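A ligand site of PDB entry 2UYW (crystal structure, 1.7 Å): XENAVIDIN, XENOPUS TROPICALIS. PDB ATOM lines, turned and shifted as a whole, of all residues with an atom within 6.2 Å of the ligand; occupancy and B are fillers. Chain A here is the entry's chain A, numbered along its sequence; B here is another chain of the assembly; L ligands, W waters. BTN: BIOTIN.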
ATOM      1  N   ASN A  14      32.109  10.954  -6.336  1.00  0.00           N
ATOM      2  CA  ASN A  14      31.319  11.939  -5.602  1.00  0.00           C
ATOM      3  C   ASN A  14      31.691  12.000  -4.137  1.00  0.00           C
ATOM      4  O   ASN A  14      32.548  11.253  -3.670  1.00  0.00           O
ATOM      5  CB  ASN A  14      29.787  11.771  -5.822  1.00  0.00           C
ATOM      6  CG  ASN A  14      29.182  10.538  -5.127  1.00  0.00           C
ATOM      7  OD1 ASN A  14      29.746   9.984  -4.170  1.00  0.00           O
ATOM      8  ND2 ASN A  14      28.002  10.120  -5.586  1.00  0.00           N
ATOM      9  N   LEU A  16      30.073  11.210  -1.443  1.00  0.00           N
ATOM     10  CA  LEU A  16      29.700  10.005  -0.688  1.00  0.00           C
ATOM     11  C   LEU A  16      30.755   8.944  -0.871  1.00  0.00           C
ATOM     12  O   LEU A  16      30.781   7.965  -0.134  1.00  0.00           O
ATOM     13  CB  LEU A  16      28.379   9.422  -1.170  1.00  0.00           C
ATOM     14  CG  LEU A  16      27.117  10.232  -0.884  1.00  0.00           C
ATOM     15  CD1 LEU A  16      25.934   9.681  -1.616  1.00  0.00           C
ATOM     16  CD2 LEU A  16      26.901  10.239   0.611  1.00  0.00           C
ATOM     17  N   GLY A  17      31.591   9.123  -1.884  1.00  0.00           N
ATOM     18  CA  GLY A  17      32.632   8.174  -2.223  1.00  0.00           C
ATOM     19  C   GLY A  17      32.199   7.149  -3.258  1.00  0.00           C
ATOM     20  O   GLY A  17      32.885   6.157  -3.434  1.00  0.00           O
ATOM     21  N   SER A  18      31.068   7.366  -3.936  1.00  0.00           N
ATOM     22  CA  SER A  18      30.646   6.449  -5.004  1.00  0.00           C
ATOM     23  C   SER A  18      31.545   6.638  -6.217  1.00  0.00           C
ATOM     24  O   SER A  18      32.044   7.750  -6.476  1.00  0.00           O
ATOM     25  CB  SER A  18      29.163   6.695  -5.370  1.00  0.00           C
ATOM     26  OG  SER A  18      28.378   6.414  -4.220  1.00  0.00           O
ATOM     27  N   ASN A  19      31.793   5.551  -6.967  1.00  0.00           N
ATOM     28  CA  ASN A  19      32.595   5.595  -8.188  1.00  0.00           C
ATOM     29  C   ASN A  19      31.744   5.500  -9.440  1.00  0.00           C
ATOM     30  O   ASN A  19      30.956   4.571  -9.597  1.00  0.00           O
ATOM     31  CB  ASN A  19      33.617   4.481  -8.200  1.00  0.00           C
ATOM     32  CG  ASN A  19      34.703   4.733  -7.214  1.00  0.00           C
ATOM     33  OD1 ASN A  19      35.476   5.682  -7.354  1.00  0.00           O
ATOM     34  ND2 ASN A  19      34.735   3.916  -6.167  1.00  0.00           N
ATOM     35  N   TYR A  35      28.552   1.937 -12.233  1.00  0.00           N
ATOM     36  CA  TYR A  35      28.452   2.723 -11.021  1.00  0.00           C
ATOM     37  C   TYR A  35      28.676   1.825  -9.824  1.00  0.00           C
ATOM     38  O   TYR A  35      28.099   0.740  -9.742  1.00  0.00           O
ATOM     39  CB  TYR A  35      27.044   3.361 -10.939  1.00  0.00           C
ATOM     40  CG  TYR A  35      27.004   4.579 -10.057  1.00  0.00           C
ATOM     41  CD1 TYR A  35      27.085   5.856 -10.614  1.00  0.00           C
ATOM     42  CD2 TYR A  35      26.869   4.468  -8.671  1.00  0.00           C
ATOM     43  CE1 TYR A  35      27.031   6.992  -9.801  1.00  0.00           C
ATOM     44  CE2 TYR A  35      26.834   5.579  -7.867  1.00  0.00           C
ATOM     45  CZ  TYR A  35      26.925   6.840  -8.445  1.00  0.00           C
ATOM     46  OH  TYR A  35      26.860   7.977  -7.666  1.00  0.00           O
ATOM     47  N   PHE A  36      29.544   2.248  -8.898  1.00  0.00           N
ATOM     48  CA  PHE A  36      29.767   1.482  -7.682  1.00  0.00           C
ATOM     49  C   PHE A  36      29.479   2.391  -6.497  1.00  0.00           C
ATOM     50  O   PHE A  36      30.306   3.209  -6.125  1.00  0.00           O
ATOM     51  CB  PHE A  36      31.194   0.939  -7.618  1.00  0.00           C
ATOM     52  CG  PHE A  36      31.379  -0.133  -6.553  1.00  0.00           C
ATOM     53  CD1 PHE A  36      30.621  -1.312  -6.579  1.00  0.00           C
ATOM     54  CD2 PHE A  36      32.331   0.026  -5.557  1.00  0.00           C
ATOM     55  CE1 PHE A  36      30.796  -2.307  -5.600  1.00  0.00           C
ATOM     56  CE2 PHE A  36      32.535  -0.993  -4.584  1.00  0.00           C
ATOM     57  CZ  PHE A  36      31.761  -2.145  -4.611  1.00  0.00           C
ATOM     58  N   THR A  37      28.279   2.269  -5.951  1.00  0.00           N
ATOM     59  CA  THR A  37      27.869   3.138  -4.860  1.00  0.00           C
ATOM     60  C   THR A  37      28.554   2.727  -3.541  1.00  0.00           C
ATOM     61  O   THR A  37      28.761   1.549  -3.274  1.00  0.00           O
ATOM     62  CB  THR A  37      26.344   3.146  -4.684  1.00  0.00           C
ATOM     63  OG1 THR A  37      26.015   4.068  -3.645  1.00  0.00           O
ATOM     64  CG2 THR A  37      25.784   1.736  -4.349  1.00  0.00           C
ATOM     65  N   SER A  38      28.915   3.711  -2.723  1.00  0.00           N
ATOM     66  CA  SER A  38      29.523   3.438  -1.417  1.00  0.00           C
ATOM     67  C   SER A  38      28.467   3.234  -0.336  1.00  0.00           C
ATOM     68  O   SER A  38      28.759   2.769   0.776  1.00  0.00           O
ATOM     69  CB  SER A  38      30.456   4.586  -1.018  1.00  0.00           C
ATOM     70  OG  SER A  38      29.697   5.780  -0.876  1.00  0.00           O
ATOM     71  N   VAL A  39      27.223   3.584  -0.680  1.00  0.00           N
ATOM     72  CA  VAL A  39      26.099   3.593   0.245  1.00  0.00           C
ATOM     73  C   VAL A  39      24.848   2.977  -0.401  1.00  0.00           C
ATOM     74  O   VAL A  39      24.693   3.020  -1.639  1.00  0.00           O
ATOM     75  CB  VAL A  39      25.763   5.043   0.706  1.00  0.00           C
ATOM     76  CG1 VAL A  39      26.947   5.620   1.516  1.00  0.00           C
ATOM     77  CG2 VAL A  39      25.430   5.947  -0.490  1.00  0.00           C
ATOM     78  N   SER A  40      23.974   2.404   0.417  1.00  0.00           N
ATOM     79  CA  SER A  40      22.718   1.848  -0.085  1.00  0.00           C
ATOM     80  C   SER A  40      21.597   1.909   0.964  1.00  0.00           C
ATOM     81  O   SER A  40      21.844   2.128   2.152  1.00  0.00           O
ATOM     82  CB  SER A  40      22.892   0.407  -0.613  1.00  0.00           C
ATOM     83  OG  SER A  40      23.270  -0.464   0.422  1.00  0.00           O
ATOM     84  N   LEU A  41      20.375   1.676   0.520  1.00  0.00           N
ATOM     85  CA  LEU A  41      19.204   1.813   1.376  1.00  0.00           C
ATOM     86  C   LEU A  41      19.065   0.739   2.451  1.00  0.00           C
ATOM     87  O   LEU A  41      18.586   1.035   3.553  1.00  0.00           O
ATOM     88  CB  LEU A  41      17.944   1.891   0.524  1.00  0.00           C
ATOM     89  CG  LEU A  41      17.739   3.182  -0.252  1.00  0.00           C
ATOM     90  CD1 LEU A  41      16.461   3.027  -1.069  1.00  0.00           C
ATOM     91  CD2 LEU A  41      17.650   4.412   0.712  1.00  0.00           C
ATOM     92  N   THR A  42      19.457  -0.492   2.111  1.00  0.00           N
ATOM     93  CA  THR A  42      19.370  -1.635   3.034  1.00  0.00           C
ATOM     94  C   THR A  42      20.749  -2.284   3.248  1.00  0.00           C
ATOM     95  O   THR A  42      21.764  -1.747   2.781  1.00  0.00           O
ATOM     96  CB  THR A  42      18.363  -2.709   2.519  1.00  0.00           C
ATOM     97  OG1 THR A  42      18.903  -3.411   1.385  1.00  0.00           O
ATOM     98  CG2 THR A  42      17.019  -2.070   2.135  1.00  0.00           C
ATOM     99  N   TRP A  69      20.367  -0.683 -10.718  1.00  0.00           N
ATOM    100  CA  TRP A  69      21.031  -1.353  -9.570  1.00  0.00           C
ATOM    101  C   TRP A  69      20.949  -2.878  -9.649  1.00  0.00           C
ATOM    102  O   TRP A  69      19.864  -3.434  -9.785  1.00  0.00           O
ATOM    103  CB  TRP A  69      20.466  -0.826  -8.248  1.00  0.00           C
ATOM    104  CG  TRP A  69      20.595   0.643  -8.111  1.00  0.00           C
ATOM    105  CD1 TRP A  69      19.571   1.577  -8.179  1.00  0.00           C
ATOM    106  CD2 TRP A  69      21.806   1.389  -7.921  1.00  0.00           C
ATOM    107  NE1 TRP A  69      20.096   2.866  -7.995  1.00  0.00           N
ATOM    108  CE2 TRP A  69      21.458   2.764  -7.842  1.00  0.00           C
ATOM    109  CE3 TRP A  69      23.167   1.010  -7.789  1.00  0.00           C
ATOM    110  CZ2 TRP A  69      22.408   3.770  -7.670  1.00  0.00           C
ATOM    111  CZ3 TRP A  69      24.120   2.015  -7.594  1.00  0.00           C
ATOM    112  CH2 TRP A  69      23.731   3.384  -7.549  1.00  0.00           C
ATOM    113  N   PHE A  71      21.593  -5.075  -7.341  1.00  0.00           N
ATOM    114  CA  PHE A  71      21.458  -5.715  -6.023  1.00  0.00           C
ATOM    115  C   PHE A  71      20.154  -5.329  -5.306  1.00  0.00           C
ATOM    116  O   PHE A  71      19.919  -5.772  -4.166  1.00  0.00           O
ATOM    117  CB  PHE A  71      22.668  -5.385  -5.136  1.00  0.00           C
ATOM    118  CG  PHE A  71      22.878  -3.914  -4.922  1.00  0.00           C
ATOM    119  CD1 PHE A  71      22.324  -3.265  -3.811  1.00  0.00           C
ATOM    120  CD2 PHE A  71      23.627  -3.167  -5.825  1.00  0.00           C
ATOM    121  CE1 PHE A  71      22.500  -1.902  -3.623  1.00  0.00           C
ATOM    122  CE2 PHE A  71      23.802  -1.783  -5.645  1.00  0.00           C
ATOM    123  CZ  PHE A  71      23.231  -1.147  -4.540  1.00  0.00           C
ATOM    124  N   SER A  72      19.342  -4.525  -5.983  1.00  0.00           N
ATOM    125  CA  SER A  72      18.046  -4.102  -5.448  1.00  0.00           C
ATOM    126  C   SER A  72      17.061  -3.847  -6.572  1.00  0.00           C
ATOM    127  O   SER A  72      17.412  -3.869  -7.746  1.00  0.00           O
ATOM    128  CB  SER A  72      18.203  -2.826  -4.616  1.00  0.00           C
ATOM    129  OG  SER A  72      18.266  -1.714  -5.476  1.00  0.00           O
ATOM    130  N   ASP A  73      15.790  -3.601  -6.203  1.00  0.00           N
ATOM    131  CA  ASP A  73      14.754  -3.336  -7.204  1.00  0.00           C
ATOM    132  C   ASP A  73      14.619  -1.852  -7.489  1.00  0.00           C
ATOM    133  O   ASP A  73      13.656  -1.433  -8.151  1.00  0.00           O
ATOM    134  CB  ASP A  73      13.402  -3.847  -6.738  1.00  0.00           C
ATOM    135  CG  ASP A  73      13.316  -5.363  -6.680  1.00  0.00           C
ATOM    136  OD1 ASP A  73      14.125  -6.072  -7.347  1.00  0.00           O
ATOM    137  OD2 ASP A  73      12.428  -5.841  -5.947  1.00  0.00           O
ATOM    138  N   SER A  74      15.590  -1.061  -7.016  1.00  0.00           N
ATOM    139  CA  SER A  74      15.550   0.385  -7.205  1.00  0.00           C
ATOM    140  C   SER A  74      16.155   0.816  -8.554  1.00  0.00           C
ATOM    141  O   SER A  74      16.821   0.016  -9.254  1.00  0.00           O
ATOM    142  CB  SER A  74      16.361   1.069  -6.099  1.00  0.00           C
ATOM    143  OG  SER A  74      15.926   0.673  -4.832  1.00  0.00           O
ATOM    144  N   THR A  76      18.044   4.655  -9.995  1.00  0.00           N
ATOM    145  CA  THR A  76      18.361   6.071  -9.811  1.00  0.00           C
ATOM    146  C   THR A  76      18.654   6.727 -11.133  1.00  0.00           C
ATOM    147  O   THR A  76      19.305   6.111 -12.001  1.00  0.00           O
ATOM    148  CB  THR A  76      19.532   6.262  -8.851  1.00  0.00           C
ATOM    149  OG1 THR A  76      19.238   5.592  -7.615  1.00  0.00           O
ATOM    150  CG2 THR A  76      19.802   7.763  -8.573  1.00  0.00           C
ATOM    151  N   TRP A  78      20.290  10.495 -12.670  1.00  0.00           N
ATOM    152  CA  TRP A  78      20.963  11.778 -12.380  1.00  0.00           C
ATOM    153  C   TRP A  78      20.829  12.677 -13.592  1.00  0.00           C
ATOM    154  O   TRP A  78      20.859  12.200 -14.747  1.00  0.00           O
ATOM    155  CB  TRP A  78      22.471  11.572 -12.179  1.00  0.00           C
ATOM    156  CG  TRP A  78      22.921  10.996 -10.890  1.00  0.00           C
ATOM    157  CD1 TRP A  78      23.510  11.665  -9.852  1.00  0.00           C
ATOM    158  CD2 TRP A  78      22.886   9.620 -10.513  1.00  0.00           C
ATOM    159  NE1 TRP A  78      23.822  10.781  -8.838  1.00  0.00           N
ATOM    160  CE2 TRP A  78      23.477   9.519  -9.229  1.00  0.00           C
ATOM    161  CE3 TRP A  78      22.429   8.445 -11.145  1.00  0.00           C
ATOM    162  CZ2 TRP A  78      23.609   8.282  -8.561  1.00  0.00           C
ATOM    163  CZ3 TRP A  78      22.563   7.230 -10.495  1.00  0.00           C
ATOM    164  CH2 TRP A  78      23.140   7.158  -9.221  1.00  0.00           C
ATOM    165  N   TRP A  96      19.574  14.064  -8.380  1.00  0.00           N
ATOM    166  CA  TRP A  96      19.189  12.669  -8.633  1.00  0.00           C
ATOM    167  C   TRP A  96      17.803  12.387  -8.039  1.00  0.00           C
ATOM    168  O   TRP A  96      17.367  13.065  -7.078  1.00  0.00           O
ATOM    169  CB  TRP A  96      20.229  11.669  -8.076  1.00  0.00           C
ATOM    170  CG  TRP A  96      20.637  11.799  -6.601  1.00  0.00           C
ATOM    171  CD1 TRP A  96      21.792  12.373  -6.095  1.00  0.00           C
ATOM    172  CD2 TRP A  96      19.927  11.279  -5.465  1.00  0.00           C
ATOM    173  NE1 TRP A  96      21.803  12.275  -4.707  1.00  0.00           N
ATOM    174  CE2 TRP A  96      20.684  11.606  -4.301  1.00  0.00           C
ATOM    175  CE3 TRP A  96      18.698  10.605  -5.312  1.00  0.00           C
ATOM    176  CZ2 TRP A  96      20.270  11.264  -2.999  1.00  0.00           C
ATOM    177  CZ3 TRP A  96      18.276  10.270  -3.991  1.00  0.00           C
ATOM    178  CH2 TRP A  96      19.070  10.588  -2.870  1.00  0.00           C
ATOM    179  N   LEU A  98      15.851   8.793  -6.758  1.00  0.00           N
ATOM    180  CA  LEU A  98      16.024   7.369  -6.464  1.00  0.00           C
ATOM    181  C   LEU A  98      14.623   6.786  -6.265  1.00  0.00           C
ATOM    182  O   LEU A  98      13.908   7.121  -5.288  1.00  0.00           O
ATOM    183  CB  LEU A  98      16.922   7.187  -5.218  1.00  0.00           C
ATOM    184  CG  LEU A  98      16.938   5.855  -4.461  1.00  0.00           C
ATOM    185  CD1 LEU A  98      17.081   4.651  -5.343  1.00  0.00           C
ATOM    186  CD2 LEU A  98      18.041   5.885  -3.355  1.00  0.00           C
ATOM    187  N   ASN A 117      24.356  15.440  -5.990  1.00  0.00           N
ATOM    188  CA  ASN A 117      25.685  14.832  -5.911  1.00  0.00           C
ATOM    189  C   ASN A 117      26.639  15.740  -6.688  1.00  0.00           C
ATOM    190  O   ASN A 117      26.240  16.335  -7.685  1.00  0.00           O
ATOM    191  CB  ASN A 117      25.736  13.448  -6.593  1.00  0.00           C
ATOM    192  CG  ASN A 117      25.251  12.298  -5.693  1.00  0.00           C
ATOM    193  OD1 ASN A 117      25.074  11.187  -6.203  1.00  0.00           O
ATOM    194  ND2 ASN A 117      25.066  12.542  -4.376  1.00  0.00           N
ATOM    195  N   PHE A 119      30.390  15.436  -8.507  1.00  0.00           N
ATOM    196  CA  PHE A 119      31.447  14.522  -8.984  1.00  0.00           C
ATOM    197  C   PHE A 119      32.668  15.290  -9.440  1.00  0.00           C
ATOM    198  O   PHE A 119      32.554  16.306 -10.124  1.00  0.00           O
ATOM    199  CB  PHE A 119      30.974  13.664 -10.164  1.00  0.00           C
ATOM    200  CG  PHE A 119      29.848  12.722  -9.831  1.00  0.00           C
ATOM    201  CD1 PHE A 119      30.124  11.423  -9.404  1.00  0.00           C
ATOM    202  CD2 PHE A 119      28.518  13.137  -9.949  1.00  0.00           C
ATOM    203  CE1 PHE A 119      29.090  10.534  -9.090  1.00  0.00           C
ATOM    204  CE2 PHE A 119      27.463  12.272  -9.617  1.00  0.00           C
ATOM    205  CZ  PHE A 119      27.731  10.962  -9.193  1.00  0.00           C
ATOM    206  N   TRP B 109      21.697  11.386   3.055  1.00  0.00           N
ATOM    207  CA  TRP B 109      21.302  11.273   1.660  1.00  0.00           C
ATOM    208  C   TRP B 109      19.985  10.513   1.479  1.00  0.00           C
ATOM    209  O   TRP B 109      19.346  10.625   0.435  1.00  0.00           O
ATOM    210  CB  TRP B 109      22.425  10.584   0.867  1.00  0.00           C
ATOM    211  CG  TRP B 109      22.643   9.093   1.228  1.00  0.00           C
ATOM    212  CD1 TRP B 109      23.445   8.580   2.219  1.00  0.00           C
ATOM    213  CD2 TRP B 109      22.016   7.971   0.596  1.00  0.00           C
ATOM    214  NE1 TRP B 109      23.361   7.192   2.223  1.00  0.00           N
ATOM    215  CE2 TRP B 109      22.468   6.808   1.253  1.00  0.00           C
ATOM    216  CE3 TRP B 109      21.056   7.855  -0.438  1.00  0.00           C
ATOM    217  CZ2 TRP B 109      22.048   5.518   0.878  1.00  0.00           C
ATOM    218  CZ3 TRP B 109      20.632   6.572  -0.803  1.00  0.00           C
ATOM    219  CH2 TRP B 109      21.113   5.426  -0.146  1.00  0.00           C
HETATM  220  C11 BTN L   1      19.535   0.908  -3.363  1.00  0.00           C
HETATM  221  O11 BTN L   1      18.455   0.273  -3.530  1.00  0.00           O
HETATM  222  O12 BTN L   1      19.952   1.106  -2.192  1.00  0.00           O
HETATM  223  C10 BTN L   1      20.330   1.381  -4.566  1.00  0.00           C
HETATM  224  C9  BTN L   1      21.541   2.261  -4.262  1.00  0.00           C
HETATM  225  C8  BTN L   1      21.168   3.757  -4.215  1.00  0.00           C
HETATM  226  C7  BTN L   1      22.368   4.645  -3.913  1.00  0.00           C
HETATM  227  C2  BTN L   1      22.093   6.143  -4.005  1.00  0.00           C
HETATM  228  S1  BTN L   1      21.813   6.709  -5.582  1.00  0.00           S
HETATM  229  C6  BTN L   1      21.919   8.415  -4.996  1.00  0.00           C
HETATM  230  C5  BTN L   1      23.040   8.424  -3.962  1.00  0.00           C
HETATM  231  N1  BTN L   1      24.280   8.729  -4.617  1.00  0.00           N
HETATM  232  C3  BTN L   1      25.127   7.691  -4.532  1.00  0.00           C
HETATM  233  O3  BTN L   1      26.395   7.739  -5.111  1.00  0.00           O
HETATM  234  N2  BTN L   1      24.594   6.664  -3.891  1.00  0.00           N
HETATM  235  C4  BTN L   1      23.234   7.007  -3.439  1.00  0.00           C
HETATM  236  O   HOH W   1      16.942  -0.953  -1.649  1.00  0.00           O
HETATM  237  O   HOH W   2      19.803  -1.735  -0.537  1.00  0.00           O
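N of Ser 18 sits at hydrogen-bond distance from OD1 of Asn 14. The side-chain hydroxyl (OG) of Ser 18 lies close to the side-chain hydroxyl (OG1) of Thr 37 (3.4 Å). The side-chain hydroxyl (OG) of Ser 18 lies within hydrogen-bond range of the backbone NH (N) of Ser 38. N of Leu 16 is in hydrogen-bond range of OD1 of Asn 14 (3.0 Å). O of Val 39 lies within hydrogen-bond range of OG1 of Thr 37. The indole nitrogen (NE1) of Trp 78 sits at hydrogen-bond distance from the side-chain amide oxygen (OD1) of Asn 117, 2.9 Å away. The indole nitrogen (NE1) of Trp 69 is in hydrogen-bond range of the side-chain hydroxyl (OG1) of Thr 76 (2.9 Å). The backbone carbonyl oxygen (O) of Leu 16 lies within hydrogen-bond range of the side-chain hydroxyl (OG) of Ser 38 (2.5 Å).
Leu 16 touches the ligand (CD1 to N1, 3.6 Å). Val 39 touches the ligand. Ser 40 touches the ligand. Trp 69 touches the ligand (CE2 to C9, 3.6 Å). Phe 71 touches the ligand (CZ to C9, 3.8 Å). CZ2 of Trp 78 touches S1 of the ligand (3.8 Å). Trp 96 touches the ligand (CE2 to C6, 3.5 Å). Leu 98 touches the ligand. CZ3 of Trp 109 of chain B touches C2 of the ligand, 3.5 Å away. Hydrophobic or aromatic side chains within 4 Å of the ligand: Leu 16, Tyr 35, Val 39, Leu 41, Trp 69, Phe 71, Trp 78, Trp 96, Leu 98 and Trp 109 of chain B.
Water W2 bridges OG1 of Thr 42 and O12 of the ligand.
OG of Ser 18 lies within hydrogen-bond range of O3 of the ligand (2.5 Å). The side-chain hydroxyl (OH) of Tyr 35 lies within hydrogen-bond range of an oxygen (O3) of the ligand, 2.6 Å away. OG of Ser 72 is in hydrogen-bond range of O11 of the ligand (2.8 Å). N of Leu 41 is in hydrogen-bond range of O12 of the ligand. The side-chain hydroxyl (OG) of Ser 74 sits at hydrogen-bond distance from an oxygen (O11) of the ligand, at 2.9 Å. The side-chain amide nitrogen (ND2) of Asn 14 lies within hydrogen-bond range of an oxygen (O3) of the ligand (2.9 Å). A nitrogen (N2) of the ligand is in hydrogen-bond range of the side-chain hydroxyl of Thr 37, 3.0 Å away. The side-chain amide oxygen (OD1) of Asn 117 is in hydrogen-bond range of a nitrogen (N1) of the ligand. OG1 of Thr 76 lies close to S1 of the ligand.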
